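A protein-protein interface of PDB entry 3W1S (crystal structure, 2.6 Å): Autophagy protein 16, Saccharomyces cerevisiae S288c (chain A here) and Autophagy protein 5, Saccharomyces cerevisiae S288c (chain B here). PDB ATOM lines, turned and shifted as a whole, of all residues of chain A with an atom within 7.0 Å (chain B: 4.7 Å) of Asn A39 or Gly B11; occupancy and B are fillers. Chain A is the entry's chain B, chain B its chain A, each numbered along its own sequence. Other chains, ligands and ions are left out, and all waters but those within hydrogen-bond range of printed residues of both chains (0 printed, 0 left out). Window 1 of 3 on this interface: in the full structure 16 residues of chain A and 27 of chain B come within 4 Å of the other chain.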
ATOM      1  N   ARG A  34     -19.926 -18.610  20.164  1.00  0.00           N
ATOM      2  CA  ARG A  34     -19.515 -17.885  18.964  1.00  0.00           C
ATOM      3  C   ARG A  34     -19.391 -18.817  17.755  1.00  0.00           C
ATOM      4  O   ARG A  34     -19.768 -18.461  16.640  1.00  0.00           O
ATOM      5  CB  ARG A  34     -18.198 -17.154  19.212  1.00  0.00           C
ATOM      6  CG  ARG A  34     -18.324 -16.142  20.302  1.00  0.00           C
ATOM      7  CD  ARG A  34     -17.189 -15.169  20.317  1.00  0.00           C
ATOM      8  NE  ARG A  34     -17.350 -14.287  21.459  1.00  0.00           N
ATOM      9  CZ  ARG A  34     -16.531 -13.296  21.763  1.00  0.00           C
ATOM     10  NH1 ARG A  34     -15.474 -13.049  21.007  1.00  0.00           N
ATOM     11  NH2 ARG A  34     -16.778 -12.549  22.825  1.00  0.00           N
ATOM     12  N   LEU A  35     -18.873 -20.018  17.991  1.00  0.00           N
ATOM     13  CA  LEU A  35     -18.723 -20.997  16.929  1.00  0.00           C
ATOM     14  C   LEU A  35     -20.100 -21.483  16.458  1.00  0.00           C
ATOM     15  O   LEU A  35     -20.323 -21.679  15.260  1.00  0.00           O
ATOM     16  CB  LEU A  35     -17.849 -22.160  17.422  1.00  0.00           C
ATOM     17  CG  LEU A  35     -16.396 -21.749  17.741  1.00  0.00           C
ATOM     18  CD1 LEU A  35     -15.629 -22.931  18.306  1.00  0.00           C
ATOM     19  CD2 LEU A  35     -15.714 -21.225  16.491  1.00  0.00           C
ATOM     20  N   THR A  36     -21.025 -21.661  17.401  1.00  0.00           N
ATOM     21  CA  THR A  36     -22.379 -22.104  17.076  1.00  0.00           C
ATOM     22  C   THR A  36     -23.039 -21.081  16.161  1.00  0.00           C
ATOM     23  O   THR A  36     -23.766 -21.441  15.242  1.00  0.00           O
ATOM     24  CB  THR A  36     -23.237 -22.272  18.348  1.00  0.00           C
ATOM     25  OG1 THR A  36     -22.730 -23.363  19.128  1.00  0.00           O
ATOM     26  CG2 THR A  36     -24.671 -22.569  17.987  1.00  0.00           C
ATOM     27  N   ASP A  37     -22.777 -19.804  16.419  1.00  0.00           N
ATOM     28  CA  ASP A  37     -23.327 -18.725  15.604  1.00  0.00           C
ATOM     29  C   ASP A  37     -22.660 -18.790  14.246  1.00  0.00           C
ATOM     30  O   ASP A  37     -23.309 -18.633  13.209  1.00  0.00           O
ATOM     31  CB  ASP A  37     -23.037 -17.340  16.213  1.00  0.00           C
ATOM     32  CG  ASP A  37     -23.803 -17.076  17.505  1.00  0.00           C
ATOM     33  OD1 ASP A  37     -24.957 -17.547  17.652  1.00  0.00           O
ATOM     34  OD2 ASP A  37     -23.245 -16.367  18.373  1.00  0.00           O
ATOM     35  N   ARG A  38     -21.348 -19.008  14.271  1.00  0.00           N
ATOM     36  CA  ARG A  38     -20.551 -19.097  13.059  1.00  0.00           C
ATOM     37  C   ARG A  38     -21.155 -20.133  12.135  1.00  0.00           C
ATOM     38  O   ARG A  38     -21.516 -19.839  10.994  1.00  0.00           O
ATOM     39  CB  ARG A  38     -19.115 -19.503  13.394  1.00  0.00           C
ATOM     40  CG  ARG A  38     -18.178 -19.497  12.190  1.00  0.00           C
ATOM     41  CD  ARG A  38     -16.891 -20.223  12.495  1.00  0.00           C
ATOM     42  NE  ARG A  38     -17.109 -21.657  12.655  1.00  0.00           N
ATOM     43  CZ  ARG A  38     -16.131 -22.547  12.770  1.00  0.00           C
ATOM     44  NH1 ARG A  38     -16.420 -23.833  12.905  1.00  0.00           N
ATOM     45  NH2 ARG A  38     -14.864 -22.151  12.752  1.00  0.00           N
ATOM     46  N   ASN A  39     -21.271 -21.353  12.636  1.00  0.00           N
ATOM     47  CA  ASN A  39     -21.826 -22.428  11.838  1.00  0.00           C
ATOM     48  C   ASN A  39     -23.194 -22.074  11.261  1.00  0.00           C
ATOM     49  O   ASN A  39     -23.452 -22.319  10.084  1.00  0.00           O
ATOM     50  CB  ASN A  39     -21.859 -23.715  12.668  1.00  0.00           C
ATOM     51  CG  ASN A  39     -20.469 -24.315  12.837  1.00  0.00           C
ATOM     52  OD1 ASN A  39     -19.478 -23.747  12.359  1.00  0.00           O
ATOM     53  ND2 ASN A  39     -20.385 -25.459  13.507  1.00  0.00           N
ATOM     54  N   ASP A  40     -24.052 -21.471  12.078  1.00  0.00           N
ATOM     55  CA  ASP A  40     -25.381 -21.070  11.629  1.00  0.00           C
ATOM     56  C   ASP A  40     -25.333 -19.932  10.600  1.00  0.00           C
ATOM     57  O   ASP A  40     -26.051 -19.969   9.599  1.00  0.00           O
ATOM     58  CB  ASP A  40     -26.237 -20.651  12.825  1.00  0.00           C
ATOM     59  CG  ASP A  40     -26.740 -21.837  13.628  1.00  0.00           C
ATOM     60  OD1 ASP A  40     -27.255 -21.622  14.750  1.00  0.00           O
ATOM     61  OD2 ASP A  40     -26.626 -22.984  13.136  1.00  0.00           O
ATOM     62  N   LYS A  41     -24.500 -18.922  10.833  1.00  0.00           N
ATOM     63  CA  LYS A  41     -24.413 -17.824   9.880  1.00  0.00           C
ATOM     64  C   LYS A  41     -23.831 -18.338   8.562  1.00  0.00           C
ATOM     65  O   LYS A  41     -24.216 -17.891   7.478  1.00  0.00           O
ATOM     66  CB  LYS A  41     -23.546 -16.694  10.439  1.00  0.00           C
ATOM     67  N   GLU A  42     -22.914 -19.293   8.658  1.00  0.00           N
ATOM     68  CA  GLU A  42     -22.274 -19.848   7.474  1.00  0.00           C
ATOM     69  C   GLU A  42     -23.125 -20.907   6.777  1.00  0.00           C
ATOM     70  O   GLU A  42     -22.891 -21.227   5.607  1.00  0.00           O
ATOM     71  CB  GLU A  42     -20.888 -20.401   7.843  1.00  0.00           C
ATOM     72  CG  GLU A  42     -19.868 -19.285   8.087  1.00  0.00           C
ATOM     73  CD  GLU A  42     -18.519 -19.762   8.622  1.00  0.00           C
ATOM     74  OE1 GLU A  42     -17.633 -18.897   8.799  1.00  0.00           O
ATOM     75  OE2 GLU A  42     -18.337 -20.978   8.866  1.00  0.00           O
ATOM     76  N   ALA A  43     -24.116 -21.437   7.489  1.00  0.00           N
ATOM     77  CA  ALA A  43     -25.003 -22.446   6.913  1.00  0.00           C
ATOM     78  C   ALA A  43     -26.238 -21.777   6.295  1.00  0.00           C
ATOM     79  O   ALA A  43     -26.984 -22.400   5.541  1.00  0.00           O
ATOM     80  CB  ALA A  43     -25.426 -23.438   7.974  1.00  0.00           C
ATOM     81  N   HIS A  44     -26.439 -20.502   6.609  1.00  0.00           N
ATOM     82  CA  HIS A  44     -27.571 -19.768   6.085  1.00  0.00           C
ATOM     83  C   HIS A  44     -27.621 -19.851   4.560  1.00  0.00           C
ATOM     84  O   HIS A  44     -26.603 -19.696   3.884  1.00  0.00           O
ATOM     85  CB  HIS A  44     -27.498 -18.305   6.531  1.00  0.00           C
ATOM     86  CG  HIS A  44     -28.654 -17.478   6.058  1.00  0.00           C
ATOM     87  ND1 HIS A  44     -29.967 -17.859   6.251  1.00  0.00           N
ATOM     88  CD2 HIS A  44     -28.696 -16.318   5.360  1.00  0.00           C
ATOM     89  CE1 HIS A  44     -30.765 -16.971   5.687  1.00  0.00           C
ATOM     90  NE2 HIS A  44     -30.020 -16.026   5.140  1.00  0.00           N
ATOM     91  N   LEU B   7     -17.798 -28.778  16.933  1.00  0.00           N
ATOM     92  CA  LEU B   7     -18.301 -27.619  16.207  1.00  0.00           C
ATOM     93  C   LEU B   7     -17.335 -27.206  15.104  1.00  0.00           C
ATOM     94  O   LEU B   7     -17.748 -26.735  14.042  1.00  0.00           O
ATOM     95  CB  LEU B   7     -18.498 -26.436  17.157  1.00  0.00           C
ATOM     96  CG  LEU B   7     -19.655 -26.491  18.151  1.00  0.00           C
ATOM     97  CD1 LEU B   7     -19.588 -25.249  19.058  1.00  0.00           C
ATOM     98  CD2 LEU B   7     -20.994 -26.569  17.382  1.00  0.00           C
ATOM     99  N   LEU B   8     -16.043 -27.361  15.370  1.00  0.00           N
ATOM    100  CA  LEU B   8     -15.031 -27.007  14.388  1.00  0.00           C
ATOM    101  C   LEU B   8     -15.036 -28.001  13.229  1.00  0.00           C
ATOM    102  O   LEU B   8     -14.828 -27.624  12.069  1.00  0.00           O
ATOM    103  CB  LEU B   8     -13.654 -26.976  15.037  1.00  0.00           C
ATOM    104  CG  LEU B   8     -13.409 -25.923  16.116  1.00  0.00           C
ATOM    105  CD1 LEU B   8     -11.937 -25.975  16.467  1.00  0.00           C
ATOM    106  CD2 LEU B   8     -13.791 -24.526  15.646  1.00  0.00           C
ATOM    107  N   TRP B   9     -15.287 -29.268  13.547  1.00  0.00           N
ATOM    108  CA  TRP B   9     -15.325 -30.315  12.533  1.00  0.00           C
ATOM    109  C   TRP B   9     -16.527 -30.136  11.631  1.00  0.00           C
ATOM    110  O   TRP B   9     -16.506 -30.561  10.487  1.00  0.00           O
ATOM    111  CB  TRP B   9     -15.396 -31.695  13.180  1.00  0.00           C
ATOM    112  CG  TRP B   9     -15.107 -32.831  12.230  1.00  0.00           C
ATOM    113  CD1 TRP B   9     -15.967 -33.823  11.855  1.00  0.00           C
ATOM    114  CD2 TRP B   9     -13.842 -33.145  11.620  1.00  0.00           C
ATOM    115  NE1 TRP B   9     -15.313 -34.740  11.063  1.00  0.00           N
ATOM    116  CE2 TRP B   9     -14.010 -34.351  10.906  1.00  0.00           C
ATOM    117  CE3 TRP B   9     -12.579 -32.528  11.623  1.00  0.00           C
ATOM    118  CZ2 TRP B   9     -12.966 -34.953  10.193  1.00  0.00           C
ATOM    119  CZ3 TRP B   9     -11.539 -33.125  10.917  1.00  0.00           C
ATOM    120  CH2 TRP B   9     -11.738 -34.330  10.214  1.00  0.00           C
ATOM    121  N   ASN B  10     -17.570 -29.502  12.160  1.00  0.00           N
ATOM    122  CA  ASN B  10     -18.797 -29.253  11.409  1.00  0.00           C
ATOM    123  C   ASN B  10     -18.750 -27.974  10.583  1.00  0.00           C
ATOM    124  O   ASN B  10     -19.580 -27.776   9.697  1.00  0.00           O
ATOM    125  CB  ASN B  10     -19.986 -29.190  12.361  1.00  0.00           C
ATOM    126  CG  ASN B  10     -20.314 -30.537  12.965  1.00  0.00           C
ATOM    127  OD1 ASN B  10     -20.967 -30.619  14.006  1.00  0.00           O
ATOM    128  ND2 ASN B  10     -19.872 -31.604  12.309  1.00  0.00           N
ATOM    129  N   GLY B  11     -17.791 -27.103  10.883  1.00  0.00           N
ATOM    130  CA  GLY B  11     -17.670 -25.866  10.130  1.00  0.00           C
ATOM    131  C   GLY B  11     -17.776 -26.137   8.639  1.00  0.00           C
ATOM    132  O   GLY B  11     -17.035 -26.960   8.090  1.00  0.00           O
ATOM    133  N   GLU B  12     -18.703 -25.450   7.980  1.00  0.00           N
ATOM    134  CA  GLU B  12     -18.903 -25.637   6.556  1.00  0.00           C
ATOM    135  C   GLU B  12     -19.275 -24.323   5.878  1.00  0.00           C
ATOM    136  O   GLU B  12     -20.049 -23.529   6.418  1.00  0.00           O
ATOM    137  CB  GLU B  12     -19.994 -26.672   6.341  1.00  0.00           C
ATOM    138  CG  GLU B  12     -20.009 -27.294   4.970  1.00  0.00           C
ATOM    139  CD  GLU B  12     -20.878 -28.533   4.939  1.00  0.00           C
ATOM    140  OE1 GLU B  12     -22.120 -28.387   4.961  1.00  0.00           O
ATOM    141  OE2 GLU B  12     -20.317 -29.654   4.916  1.00  0.00           O
ATOM    142  N   LEU B  13     -18.722 -24.099   4.690  1.00  0.00           N
ATOM    143  CA  LEU B  13     -18.978 -22.876   3.944  1.00  0.00           C
ATOM    144  C   LEU B  13     -19.670 -23.149   2.611  1.00  0.00           C
ATOM    145  O   LEU B  13     -19.624 -24.266   2.097  1.00  0.00           O
ATOM    146  CB  LEU B  13     -17.662 -22.152   3.662  1.00  0.00           C
ATOM    147  CG  LEU B  13     -16.729 -21.769   4.813  1.00  0.00           C
ATOM    148  CD1 LEU B  13     -15.400 -21.316   4.217  1.00  0.00           C
ATOM    149  CD2 LEU B  13     -17.343 -20.668   5.671  1.00  0.00           C
ATOM    150  N   VAL B  39     -18.318 -26.929   1.357  1.00  0.00           N
ATOM    151  CA  VAL B  39     -16.972 -27.368   1.696  1.00  0.00           C
ATOM    152  C   VAL B  39     -16.650 -27.108   3.163  1.00  0.00           C
ATOM    153  O   VAL B  39     -16.892 -26.011   3.672  1.00  0.00           O
ATOM    154  CB  VAL B  39     -15.933 -26.633   0.829  1.00  0.00           C
ATOM    155  CG1 VAL B  39     -14.530 -27.089   1.189  1.00  0.00           C
ATOM    156  CG2 VAL B  39     -16.223 -26.881  -0.645  1.00  0.00           C
ATOM    157  N   PRO B  40     -16.102 -28.116   3.869  1.00  0.00           N
ATOM    158  CA  PRO B  40     -15.746 -27.967   5.289  1.00  0.00           C
ATOM    159  C   PRO B  40     -14.643 -26.931   5.491  1.00  0.00           C
ATOM    160  O   PRO B  40     -13.900 -26.613   4.566  1.00  0.00           O
ATOM    161  CB  PRO B  40     -15.277 -29.374   5.682  1.00  0.00           C
ATOM    162  CG  PRO B  40     -16.045 -30.259   4.755  1.00  0.00           C
ATOM    163  CD  PRO B  40     -15.944 -29.515   3.442  1.00  0.00           C
ATOM    164  N   ARG B  41     -14.544 -26.398   6.703  1.00  0.00           N
ATOM    165  CA  ARG B  41     -13.508 -25.422   7.014  1.00  0.00           C
ATOM    166  C   ARG B  41     -12.192 -26.181   7.192  1.00  0.00           C
ATOM    167  O   ARG B  41     -11.123 -25.723   6.775  1.00  0.00           O
ATOM    168  CB  ARG B  41     -13.840 -24.691   8.320  1.00  0.00           C
ATOM    169  CG  ARG B  41     -14.673 -23.427   8.171  1.00  0.00           C
ATOM    170  CD  ARG B  41     -14.974 -22.792   9.525  1.00  0.00           C
ATOM    171  NE  ARG B  41     -15.407 -21.404   9.380  1.00  0.00           N
ATOM    172  CZ  ARG B  41     -14.584 -20.359   9.321  1.00  0.00           C
ATOM    173  NH1 ARG B  41     -15.069 -19.132   9.176  1.00  0.00           N
ATOM    174  NH2 ARG B  41     -13.277 -20.534   9.431  1.00  0.00           N
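The guanidinium group (NH1) of Arg A38 sits at hydrogen-bond distance from the side-chain amide oxygen (OD1) of Asn A39 (3.1 Å).
The backbone carbonyl oxygen of Val B39 is in hydrogen-bond range of the backbone NH of Leu B13, 2.8 Å away.
The backbone NH (N) of Arg B41 is in hydrogen-bond range of the backbone carbonyl oxygen (O) of Gly B11 (2.9 Å).
CD1 of Leu B7 touches CB of Leu A35 (3.9 Å).
Leu A35 touches Leu B8.
Leu B7 touches Thr A36 (CD1 to OG1, 3.7 Å).
Arg A38 touches Leu B8 (NH1 to CA, 3.8 Å).
Arg A38 touches Gly B11 (NH1 to CA, 3.7 Å).
Asn A39 touches Asn B10.
Asn A39 touches Gly B11 (OD1 to CA, 3.6 Å).
CB of Glu A42 touches O of Glu B12, 3.5 Å away.
Glu A42 touches Leu B13 (CD to CD2, 3.3 Å).
Hydrophobic or aromatic side chains of chain B that line the printed part of chain A: Leu B7, Leu B8 and Leu B13.
Hydrophobic or aromatic side chains of chain A within 4 Å of the printed part of chain B: Leu A35.
Among the printed residues, 13 pairs touch across the chains.
The guanidinium group (NE) of Arg B41 lies close to the guanidinium group (NH2) of Arg A38 (3.5 Å).
O of Leu B7 is in hydrogen-bond range of NH1 of Arg A38, 3.4 Å away.
The side-chain carboxylate (OE1) of Glu A42 is in salt-bridge range of the guanidinium group (NH1) of Arg B41.
The side-chain amide nitrogen (ND2) of Asn A39 sits at hydrogen-bond distance from the backbone carbonyl oxygen (O) of Leu B7 (3.0 Å).
Arg A34 touches none of the printed residues of chain B.
Of the printed residues of chain B, Asn A39 touches Leu B7, Asn B10 and Gly B11.
Ala A43 touches none of the printed residues of chain B.
Of the printed residues of chain A, Leu B7 touches Leu A35, Thr A36, Arg A38 and Asn A39.
Of the printed residues of chain A, Leu B8 touches Leu A35 (3.6 Å) and Arg A38 (3.8 Å).
Of the printed residues of chain A, Asn B10 touches Asn A39 (3.9 Å).
Of chain A, only Arg A38 and Asn A39 come within 4 Å of Gly B11.
Printed residues of chain A within 4 Å of Arg B41: Arg A38 (3.3 Å) and Glu A42 (2.6 Å).
The nearest residue of chain A that does not touch Gly B11 is Glu A42 (5.1 Å).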
